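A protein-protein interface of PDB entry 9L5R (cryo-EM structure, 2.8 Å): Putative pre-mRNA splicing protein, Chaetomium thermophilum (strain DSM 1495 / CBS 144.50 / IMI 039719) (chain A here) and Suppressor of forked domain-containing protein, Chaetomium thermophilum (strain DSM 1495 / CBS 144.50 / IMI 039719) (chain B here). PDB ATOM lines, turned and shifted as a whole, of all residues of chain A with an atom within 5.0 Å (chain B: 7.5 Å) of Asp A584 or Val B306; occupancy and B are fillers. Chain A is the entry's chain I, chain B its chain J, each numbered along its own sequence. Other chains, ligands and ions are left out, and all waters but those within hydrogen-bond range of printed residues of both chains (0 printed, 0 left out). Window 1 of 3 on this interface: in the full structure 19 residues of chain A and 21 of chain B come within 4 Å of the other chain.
Of the printed residues of chain B, Glu A580 touches Arg B310 (3.1 Å) and Leu B334 (3.7 Å).
Asp A584 touches just these residues of chain B: Thr B290 (3.6 Å), Lys B294 (3.6 Å), Val B306 (3.97 Å) and Lys B309 (3.3 Å).
Of the printed residues of chain A, Thr B290 touches Asp A584.
Printed residues of chain A within 4 Å of Thr B291: Gln A588.
Of the printed residues of chain A, Glu B303 touches Arg A581 (3.1 Å).
Of chain A, only Arg A581 and Asp A584 come within 4 Å of Val B306.
The nearest residue of chain B that does not touch Asp A584 is Arg B310 (4.4 Å).
Hydrophobic or aromatic side chains of chain A that line the printed part of chain B: Leu A585.
Of the 21 printed residues of chain B, 9 touch a printed residue of chain A.
Along chain B the printed residues that touch a printed residue of chain A span positions 290 to 334.
Among the printed residues, merely in contact across the chains: Asp A584 with Lys B309 (3.3 Å), Gln A588 with Thr B291 (3.4 Å), Asp A584 with Thr B290 (3.6 Å), Glu A580 with Leu B334 (3.7 Å), Arg A583 with Arg B310 (3.7 Å), Arg A581 with Val B306 (3.9 Å), Leu A585 with Lys B294 (3.97 Å), Asp A584 with Val B306 (3.97 Å) and Arg A581 with Val B302 (3.97 Å).
The side-chain hydroxyl (OG1) of Thr B291 sits at hydrogen-bond distance from the backbone carbonyl oxygen (O) of Ala B287, at 3.3 Å.
The guanidinium group (NH1) of Arg A583 is in salt-bridge range of the side-chain carboxylate (OE2) of Glu A580 (2.4 Å).
The backbone carbonyl oxygen (O) of His B286 lies within hydrogen-bond range of the side-chain hydroxyl (OG1) of Thr B290, 2.7 Å away.
OE1 of Gln A588 lies within hydrogen-bond range of NZ of Lys B294 (2.6 Å).
NH1 of Arg A581 lies within salt-bridge range of OE2 of Glu B303 (3.1 Å).
The side-chain carboxylate (OD2) of Asp A584 lies within salt-bridge range of the side-chain amino group (NZ) of Lys B294 (3.6 Å).
NE of Arg B310 lies within salt-bridge range of OE1 of Glu A580, at 3.1 Å.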
ATOM      1  N   ILE A 579       7.187   9.575  -9.301  1.00  0.00           N
ATOM      2  CA  ILE A 579       7.318  10.774 -10.123  1.00  0.00           C
ATOM      3  C   ILE A 579       8.640  11.481  -9.855  1.00  0.00           C
ATOM      4  O   ILE A 579       9.262  12.014 -10.778  1.00  0.00           O
ATOM      5  CB  ILE A 579       6.100  11.697  -9.907  1.00  0.00           C
ATOM      6  CG1 ILE A 579       6.241  13.002 -10.692  1.00  0.00           C
ATOM      7  CG2 ILE A 579       5.866  11.971  -8.430  1.00  0.00           C
ATOM      8  CD1 ILE A 579       6.207  12.816 -12.185  1.00  0.00           C
ATOM      9  N   GLU A 580       9.116  11.467  -8.607  1.00  0.00           N
ATOM     10  CA  GLU A 580      10.417  12.055  -8.309  1.00  0.00           C
ATOM     11  C   GLU A 580      11.543  11.242  -8.932  1.00  0.00           C
ATOM     12  O   GLU A 580      12.541  11.802  -9.400  1.00  0.00           O
ATOM     13  CB  GLU A 580      10.598  12.161  -6.801  1.00  0.00           C
ATOM     14  CG  GLU A 580       9.539  13.002  -6.130  1.00  0.00           C
ATOM     15  CD  GLU A 580       9.580  14.443  -6.573  1.00  0.00           C
ATOM     16  OE1 GLU A 580      10.692  14.981  -6.745  1.00  0.00           O
ATOM     17  OE2 GLU A 580       8.501  15.043  -6.742  1.00  0.00           O
ATOM     18  N   ARG A 581      11.386   9.923  -8.964  1.00  0.00           N
ATOM     19  CA  ARG A 581      12.362   9.056  -9.612  1.00  0.00           C
ATOM     20  C   ARG A 581      12.419   9.314 -11.116  1.00  0.00           C
ATOM     21  O   ARG A 581      13.507   9.409 -11.702  1.00  0.00           O
ATOM     22  CB  ARG A 581      11.997   7.610  -9.292  1.00  0.00           C
ATOM     23  CG  ARG A 581      12.972   6.561  -9.719  1.00  0.00           C
ATOM     24  CD  ARG A 581      12.521   5.221  -9.176  1.00  0.00           C
ATOM     25  NE  ARG A 581      13.252   4.118  -9.778  1.00  0.00           N
ATOM     26  CZ  ARG A 581      13.016   2.842  -9.521  1.00  0.00           C
ATOM     27  NH1 ARG A 581      12.100   2.474  -8.644  1.00  0.00           N
ATOM     28  NH2 ARG A 581      13.711   1.911 -10.164  1.00  0.00           N
ATOM     29  N   LEU A 582      11.255   9.470 -11.751  1.00  0.00           N
ATOM     30  CA  LEU A 582      11.202   9.796 -13.172  1.00  0.00           C
ATOM     31  C   LEU A 582      11.748  11.186 -13.465  1.00  0.00           C
ATOM     32  O   LEU A 582      12.411  11.385 -14.492  1.00  0.00           O
ATOM     33  CB  LEU A 582       9.767   9.694 -13.678  1.00  0.00           C
ATOM     34  CG  LEU A 582       9.318   8.299 -14.095  1.00  0.00           C
ATOM     35  CD1 LEU A 582       7.852   8.295 -14.468  1.00  0.00           C
ATOM     36  CD2 LEU A 582      10.166   7.790 -15.237  1.00  0.00           C
ATOM     37  N   ARG A 583      11.479  12.147 -12.585  1.00  0.00           N
ATOM     38  CA  ARG A 583      12.069  13.471 -12.701  1.00  0.00           C
ATOM     39  C   ARG A 583      13.584  13.416 -12.620  1.00  0.00           C
ATOM     40  O   ARG A 583      14.263  14.109 -13.383  1.00  0.00           O
ATOM     41  CB  ARG A 583      11.529  14.382 -11.602  1.00  0.00           C
ATOM     42  CG  ARG A 583      10.244  15.085 -11.959  1.00  0.00           C
ATOM     43  CD  ARG A 583       9.737  15.906 -10.797  1.00  0.00           C
ATOM     44  NE  ARG A 583       8.360  16.332 -10.999  1.00  0.00           N
ATOM     45  CZ  ARG A 583       7.447  16.380 -10.041  1.00  0.00           C
ATOM     46  NH1 ARG A 583       7.731  16.027  -8.800  1.00  0.00           N
ATOM     47  NH2 ARG A 583       6.219  16.792 -10.335  1.00  0.00           N
ATOM     48  N   ASP A 584      14.117  12.592 -11.718  1.00  0.00           N
ATOM     49  CA  ASP A 584      15.560  12.419 -11.618  1.00  0.00           C
ATOM     50  C   ASP A 584      16.136  11.822 -12.895  1.00  0.00           C
ATOM     51  O   ASP A 584      17.200  12.247 -13.359  1.00  0.00           O
ATOM     52  CB  ASP A 584      15.898  11.541 -10.418  1.00  0.00           C
ATOM     53  CG  ASP A 584      17.310  11.741  -9.944  1.00  0.00           C
ATOM     54  OD1 ASP A 584      17.810  12.876 -10.057  1.00  0.00           O
ATOM     55  OD2 ASP A 584      17.924  10.769  -9.466  1.00  0.00           O
ATOM     56  N   LEU A 585      15.441  10.841 -13.480  1.00  0.00           N
ATOM     57  CA  LEU A 585      15.887  10.270 -14.751  1.00  0.00           C
ATOM     58  C   LEU A 585      15.923  11.313 -15.858  1.00  0.00           C
ATOM     59  O   LEU A 585      16.865  11.362 -16.661  1.00  0.00           O
ATOM     60  CB  LEU A 585      14.968   9.131 -15.174  1.00  0.00           C
ATOM     61  CG  LEU A 585      15.058   7.793 -14.470  1.00  0.00           C
ATOM     62  CD1 LEU A 585      14.300   6.789 -15.294  1.00  0.00           C
ATOM     63  CD2 LEU A 585      16.494   7.382 -14.314  1.00  0.00           C
ATOM     64  N   PHE A 586      14.896  12.153 -15.925  1.00  0.00           N
ATOM     65  CA  PHE A 586      14.842  13.121 -17.011  1.00  0.00           C
ATOM     66  C   PHE A 586      15.886  14.213 -16.831  1.00  0.00           C
ATOM     67  O   PHE A 586      16.496  14.655 -17.812  1.00  0.00           O
ATOM     68  CB  PHE A 586      13.439  13.698 -17.125  1.00  0.00           C
ATOM     69  CG  PHE A 586      12.552  12.918 -18.041  1.00  0.00           C
ATOM     70  CD1 PHE A 586      12.636  13.084 -19.407  1.00  0.00           C
ATOM     71  CD2 PHE A 586      11.659  11.997 -17.538  1.00  0.00           C
ATOM     72  CE1 PHE A 586      11.832  12.363 -20.254  1.00  0.00           C
ATOM     73  CE2 PHE A 586      10.853  11.271 -18.380  1.00  0.00           C
ATOM     74  CZ  PHE A 586      10.940  11.454 -19.738  1.00  0.00           C
ATOM     75  N   GLU A 587      16.135  14.639 -15.589  1.00  0.00           N
ATOM     76  CA  GLU A 587      17.247  15.557 -15.354  1.00  0.00           C
ATOM     77  C   GLU A 587      18.584  14.908 -15.680  1.00  0.00           C
ATOM     78  O   GLU A 587      19.496  15.582 -16.168  1.00  0.00           O
ATOM     79  CB  GLU A 587      17.252  16.057 -13.912  1.00  0.00           C
ATOM     80  CG  GLU A 587      15.990  16.758 -13.471  1.00  0.00           C
ATOM     81  CD  GLU A 587      15.960  18.206 -13.878  1.00  0.00           C
ATOM     82  OE1 GLU A 587      17.020  18.859 -13.819  1.00  0.00           O
ATOM     83  OE2 GLU A 587      14.874  18.698 -14.251  1.00  0.00           O
ATOM     84  N   GLN A 588      18.711  13.604 -15.437  1.00  0.00           N
ATOM     85  CA  GLN A 588      19.947  12.889 -15.728  1.00  0.00           C
ATOM     86  C   GLN A 588      20.230  12.832 -17.227  1.00  0.00           C
ATOM     87  O   GLN A 588      21.387  12.930 -17.644  1.00  0.00           O
ATOM     88  CB  GLN A 588      19.865  11.490 -15.122  1.00  0.00           C
ATOM     89  CG  GLN A 588      21.006  10.568 -15.440  1.00  0.00           C
ATOM     90  CD  GLN A 588      20.976   9.335 -14.578  1.00  0.00           C
ATOM     91  OE1 GLN A 588      21.235   9.401 -13.381  1.00  0.00           O
ATOM     92  NE2 GLN A 588      20.651   8.199 -15.177  1.00  0.00           N
ATOM     93  N   HIS B 286      27.127  13.020  -3.880  1.00  0.00           N
ATOM     94  CA  HIS B 286      25.775  12.489  -3.753  1.00  0.00           C
ATOM     95  C   HIS B 286      25.175  12.138  -5.106  1.00  0.00           C
ATOM     96  O   HIS B 286      24.427  11.162  -5.217  1.00  0.00           O
ATOM     97  CB  HIS B 286      24.870  13.468  -3.020  1.00  0.00           C
ATOM     98  CG  HIS B 286      23.730  12.800  -2.320  1.00  0.00           C
ATOM     99  ND1 HIS B 286      22.705  12.182  -3.002  1.00  0.00           N
ATOM    100  CD2 HIS B 286      23.471  12.616  -1.006  1.00  0.00           C
ATOM    101  CE1 HIS B 286      21.855  11.662  -2.136  1.00  0.00           C
ATOM    102  NE2 HIS B 286      22.297  11.911  -0.917  1.00  0.00           N
ATOM    103  N   ALA B 287      25.471  12.931  -6.138  1.00  0.00           N
ATOM    104  CA  ALA B 287      24.978  12.600  -7.475  1.00  0.00           C
ATOM    105  C   ALA B 287      25.545  11.271  -7.962  1.00  0.00           C
ATOM    106  O   ALA B 287      24.818  10.430  -8.516  1.00  0.00           O
ATOM    107  CB  ALA B 287      25.323  13.718  -8.453  1.00  0.00           C
ATOM    108  N   THR B 290      23.865   8.453  -6.102  1.00  0.00           N
ATOM    109  CA  THR B 290      22.542   8.178  -6.650  1.00  0.00           C
ATOM    110  C   THR B 290      22.629   7.319  -7.900  1.00  0.00           C
ATOM    111  O   THR B 290      21.892   6.336  -8.044  1.00  0.00           O
ATOM    112  CB  THR B 290      21.829   9.486  -6.957  1.00  0.00           C
ATOM    113  OG1 THR B 290      21.880  10.327  -5.802  1.00  0.00           O
ATOM    114  CG2 THR B 290      20.392   9.225  -7.315  1.00  0.00           C
ATOM    115  N   THR B 291      23.542   7.666  -8.810  1.00  0.00           N
ATOM    116  CA  THR B 291      23.713   6.848 -10.008  1.00  0.00           C
ATOM    117  C   THR B 291      24.228   5.455  -9.661  1.00  0.00           C
ATOM    118  O   THR B 291      23.839   4.466 -10.294  1.00  0.00           O
ATOM    119  CB  THR B 291      24.651   7.541 -10.988  1.00  0.00           C
ATOM    120  OG1 THR B 291      25.883   7.856 -10.335  1.00  0.00           O
ATOM    121  CG2 THR B 291      24.024   8.812 -11.496  1.00  0.00           C
ATOM    122  N   GLU B 293      23.574   3.725  -6.871  1.00  0.00           N
ATOM    123  CA  GLU B 293      22.489   2.914  -6.337  1.00  0.00           C
ATOM    124  C   GLU B 293      21.475   2.563  -7.409  1.00  0.00           C
ATOM    125  O   GLU B 293      20.887   1.479  -7.364  1.00  0.00           O
ATOM    126  CB  GLU B 293      21.811   3.626  -5.176  1.00  0.00           C
ATOM    127  CG  GLU B 293      22.713   3.841  -3.993  1.00  0.00           C
ATOM    128  CD  GLU B 293      22.723   2.680  -3.020  1.00  0.00           C
ATOM    129  OE1 GLU B 293      22.474   1.533  -3.432  1.00  0.00           O
ATOM    130  OE2 GLU B 293      22.986   2.913  -1.826  1.00  0.00           O
ATOM    131  N   LYS B 294      21.262   3.454  -8.378  1.00  0.00           N
ATOM    132  CA  LYS B 294      20.420   3.099  -9.514  1.00  0.00           C
ATOM    133  C   LYS B 294      21.046   1.997 -10.351  1.00  0.00           C
ATOM    134  O   LYS B 294      20.331   1.249 -11.018  1.00  0.00           O
ATOM    135  CB  LYS B 294      20.156   4.326 -10.377  1.00  0.00           C
ATOM    136  CG  LYS B 294      19.227   5.324  -9.746  1.00  0.00           C
ATOM    137  CD  LYS B 294      18.741   6.329 -10.760  1.00  0.00           C
ATOM    138  CE  LYS B 294      19.464   7.644 -10.606  1.00  0.00           C
ATOM    139  NZ  LYS B 294      19.404   8.457 -11.841  1.00  0.00           N
ATOM    140  N   GLU B 300      14.767  -0.302  -2.401  1.00  0.00           N
ATOM    141  CA  GLU B 300      14.585   0.602  -1.270  1.00  0.00           C
ATOM    142  C   GLU B 300      15.750   1.571  -1.137  1.00  0.00           C
ATOM    143  O   GLU B 300      15.543   2.746  -0.816  1.00  0.00           O
ATOM    144  CB  GLU B 300      14.387  -0.194   0.017  1.00  0.00           C
ATOM    145  CG  GLU B 300      15.365  -1.331   0.208  1.00  0.00           C
ATOM    146  CD  GLU B 300      14.798  -2.660  -0.245  1.00  0.00           C
ATOM    147  OE1 GLU B 300      13.871  -2.655  -1.080  1.00  0.00           O
ATOM    148  OE2 GLU B 300      15.274  -3.708   0.240  1.00  0.00           O
ATOM    149  N   GLY B 301      16.967   1.114  -1.429  1.00  0.00           N
ATOM    150  CA  GLY B 301      18.091   2.031  -1.508  1.00  0.00           C
ATOM    151  C   GLY B 301      17.939   3.045  -2.625  1.00  0.00           C
ATOM    152  O   GLY B 301      18.349   4.201  -2.483  1.00  0.00           O
ATOM    153  N   VAL B 302      17.336   2.628  -3.745  1.00  0.00           N
ATOM    154  CA  VAL B 302      17.132   3.548  -4.864  1.00  0.00           C
ATOM    155  C   VAL B 302      16.189   4.680  -4.473  1.00  0.00           C
ATOM    156  O   VAL B 302      16.522   5.857  -4.647  1.00  0.00           O
ATOM    157  CB  VAL B 302      16.627   2.801  -6.109  1.00  0.00           C
ATOM    158  CG1 VAL B 302      16.238   3.789  -7.181  1.00  0.00           C
ATOM    159  CG2 VAL B 302      17.691   1.881  -6.635  1.00  0.00           C
ATOM    160  N   GLU B 303      15.008   4.358  -3.917  1.00  0.00           N
ATOM    161  CA  GLU B 303      14.161   5.487  -3.505  1.00  0.00           C
ATOM    162  C   GLU B 303      14.703   6.219  -2.287  1.00  0.00           C
ATOM    163  O   GLU B 303      14.389   7.396  -2.118  1.00  0.00           O
ATOM    164  CB  GLU B 303      12.670   5.187  -3.241  1.00  0.00           C
ATOM    165  CG  GLU B 303      11.741   4.802  -4.412  1.00  0.00           C
ATOM    166  CD  GLU B 303      11.736   3.364  -4.809  1.00  0.00           C
ATOM    167  OE1 GLU B 303      12.401   2.579  -4.141  1.00  0.00           O
ATOM    168  OE2 GLU B 303      11.050   3.020  -5.793  1.00  0.00           O
ATOM    169  N   ASP B 304      15.548   5.589  -1.466  1.00  0.00           N
ATOM    170  CA  ASP B 304      16.149   6.326  -0.357  1.00  0.00           C
ATOM    171  C   ASP B 304      17.076   7.412  -0.896  1.00  0.00           C
ATOM    172  O   ASP B 304      16.966   8.588  -0.513  1.00  0.00           O
ATOM    173  CB  ASP B 304      16.872   5.321   0.562  1.00  0.00           C
ATOM    174  CG  ASP B 304      17.778   5.957   1.652  1.00  0.00           C
ATOM    175  OD1 ASP B 304      17.949   7.185   1.797  1.00  0.00           O
ATOM    176  OD2 ASP B 304      18.353   5.155   2.416  1.00  0.00           O
ATOM    177  N   VAL B 305      17.970   7.048  -1.815  1.00  0.00           N
ATOM    178  CA  VAL B 305      18.923   8.033  -2.309  1.00  0.00           C
ATOM    179  C   VAL B 305      18.250   9.040  -3.246  1.00  0.00           C
ATOM    180  O   VAL B 305      18.625  10.219  -3.255  1.00  0.00           O
ATOM    181  CB  VAL B 305      20.137   7.325  -2.946  1.00  0.00           C
ATOM    182  CG1 VAL B 305      19.775   6.613  -4.235  1.00  0.00           C
ATOM    183  CG2 VAL B 305      21.270   8.302  -3.152  1.00  0.00           C
ATOM    184  N   VAL B 306      17.224   8.629  -4.001  1.00  0.00           N
ATOM    185  CA  VAL B 306      16.484   9.594  -4.811  1.00  0.00           C
ATOM    186  C   VAL B 306      15.702  10.551  -3.919  1.00  0.00           C
ATOM    187  O   VAL B 306      15.610  11.748  -4.216  1.00  0.00           O
ATOM    188  CB  VAL B 306      15.579   8.864  -5.825  1.00  0.00           C
ATOM    189  CG1 VAL B 306      14.660   9.828  -6.523  1.00  0.00           C
ATOM    190  CG2 VAL B 306      16.420   8.175  -6.867  1.00  0.00           C
ATOM    191  N   LEU B 307      15.163  10.057  -2.799  1.00  0.00           N
ATOM    192  CA  LEU B 307      14.490  10.920  -1.837  1.00  0.00           C
ATOM    193  C   LEU B 307      15.441  11.965  -1.278  1.00  0.00           C
ATOM    194  O   LEU B 307      15.102  13.150  -1.221  1.00  0.00           O
ATOM    195  CB  LEU B 307      13.900  10.065  -0.713  1.00  0.00           C
ATOM    196  CG  LEU B 307      13.446  10.704   0.601  1.00  0.00           C
ATOM    197  CD1 LEU B 307      12.368  11.739   0.385  1.00  0.00           C
ATOM    198  CD2 LEU B 307      12.956   9.630   1.552  1.00  0.00           C
ATOM    199  N   THR B 308      16.651  11.549  -0.898  1.00  0.00           N
ATOM    200  CA  THR B 308      17.617  12.512  -0.369  1.00  0.00           C
ATOM    201  C   THR B 308      18.040  13.528  -1.430  1.00  0.00           C
ATOM    202  O   THR B 308      18.138  14.730  -1.143  1.00  0.00           O
ATOM    203  CB  THR B 308      18.836  11.788   0.190  1.00  0.00           C
ATOM    204  OG1 THR B 308      18.408  10.666   0.968  1.00  0.00           O
ATOM    205  CG2 THR B 308      19.629  12.718   1.076  1.00  0.00           C
ATOM    206  N   LYS B 309      18.258  13.066  -2.665  1.00  0.00           N
ATOM    207  CA  LYS B 309      18.701  13.949  -3.741  1.00  0.00           C
ATOM    208  C   LYS B 309      17.640  14.986  -4.088  1.00  0.00           C
ATOM    209  O   LYS B 309      17.931  16.189  -4.168  1.00  0.00           O
ATOM    210  CB  LYS B 309      19.061  13.110  -4.968  1.00  0.00           C
ATOM    211  CG  LYS B 309      19.594  13.892  -6.151  1.00  0.00           C
ATOM    212  CD  LYS B 309      20.119  12.955  -7.225  1.00  0.00           C
ATOM    213  CE  LYS B 309      20.578  13.714  -8.455  1.00  0.00           C
ATOM    214  NZ  LYS B 309      21.741  14.582  -8.170  1.00  0.00           N
ATOM    215  N   ARG B 310      16.397  14.542  -4.281  1.00  0.00           N
ATOM    216  CA  ARG B 310      15.321  15.468  -4.607  1.00  0.00           C
ATOM    217  C   ARG B 310      14.980  16.365  -3.430  1.00  0.00           C
ATOM    218  O   ARG B 310      14.585  17.517  -3.636  1.00  0.00           O
ATOM    219  CB  ARG B 310      14.082  14.703  -5.060  1.00  0.00           C
ATOM    220  CG  ARG B 310      14.294  13.820  -6.267  1.00  0.00           C
ATOM    221  CD  ARG B 310      14.628  14.608  -7.508  1.00  0.00           C
ATOM    222  NE  ARG B 310      13.586  15.568  -7.841  1.00  0.00           N
ATOM    223  CZ  ARG B 310      13.669  16.432  -8.841  1.00  0.00           C
ATOM    224  NH1 ARG B 310      14.706  16.444  -9.658  1.00  0.00           N
ATOM    225  NH2 ARG B 310      12.679  17.297  -9.034  1.00  0.00           N
ATOM    226  N   ARG B 311      15.134  15.866  -2.199  1.00  0.00           N
ATOM    227  CA  ARG B 311      14.924  16.700  -1.023  1.00  0.00           C
ATOM    228  C   ARG B 311      15.913  17.853  -0.993  1.00  0.00           C
ATOM    229  O   ARG B 311      15.532  19.006  -0.760  1.00  0.00           O
ATOM    230  CB  ARG B 311      15.046  15.848   0.239  1.00  0.00           C
ATOM    231  CG  ARG B 311      15.381  16.628   1.489  1.00  0.00           C
ATOM    232  CD  ARG B 311      15.553  15.707   2.675  1.00  0.00           C
ATOM    233  NE  ARG B 311      14.491  14.714   2.750  1.00  0.00           N
ATOM    234  CZ  ARG B 311      14.610  13.537   3.347  1.00  0.00           C
ATOM    235  NH1 ARG B 311      15.743  13.165   3.916  1.00  0.00           N
ATOM    236  NH2 ARG B 311      13.567  12.715   3.376  1.00  0.00           N
ATOM    237  N   ARG B 312      17.186  17.565  -1.270  1.00  0.00           N
ATOM    238  CA  ARG B 312      18.180  18.632  -1.315  1.00  0.00           C
ATOM    239  C   ARG B 312      17.929  19.601  -2.465  1.00  0.00           C
ATOM    240  O   ARG B 312      18.089  20.817  -2.289  1.00  0.00           O
ATOM    241  CB  ARG B 312      19.581  18.037  -1.413  1.00  0.00           C
ATOM    242  CG  ARG B 312      20.683  19.067  -1.325  1.00  0.00           C
ATOM    243  CD  ARG B 312      21.902  18.609  -2.095  1.00  0.00           C
ATOM    244  NE  ARG B 312      22.339  17.275  -1.704  1.00  0.00           N
ATOM    245  CZ  ARG B 312      23.533  17.004  -1.194  1.00  0.00           C
ATOM    246  NH1 ARG B 312      24.458  17.939  -1.068  1.00  0.00           N
ATOM    247  NH2 ARG B 312      23.805  15.763  -0.804  1.00  0.00           N
ATOM    248  N   LEU B 313      17.527  19.093  -3.634  1.00  0.00           N
ATOM    249  CA  LEU B 313      17.242  19.975  -4.766  1.00  0.00           C
ATOM    250  C   LEU B 313      16.082  20.918  -4.464  1.00  0.00           C
ATOM    251  O   LEU B 313      16.167  22.128  -4.719  1.00  0.00           O
ATOM    252  CB  LEU B 313      16.932  19.152  -6.014  1.00  0.00           C
ATOM    253  CG  LEU B 313      16.658  19.968  -7.278  1.00  0.00           C
ATOM    254  CD1 LEU B 313      17.788  20.944  -7.553  1.00  0.00           C
ATOM    255  CD2 LEU B 313      16.437  19.064  -8.471  1.00  0.00           C
ATOM    256  N   LEU B 334       6.788  14.725  -2.173  1.00  0.00           N
ATOM    257  CA  LEU B 334       8.009  13.967  -1.924  1.00  0.00           C
ATOM    258  C   LEU B 334       8.084  13.514  -0.475  1.00  0.00           C
ATOM    259  O   LEU B 334       8.372  12.346  -0.191  1.00  0.00           O
ATOM    260  CB  LEU B 334       9.229  14.815  -2.276  1.00  0.00           C
ATOM    261  CG  LEU B 334      10.585  14.196  -1.933  1.00  0.00           C
ATOM    262  CD1 LEU B 334      10.798  12.906  -2.701  1.00  0.00           C
ATOM    263  CD2 LEU B 334      11.705  15.172  -2.195  1.00  0.00           C
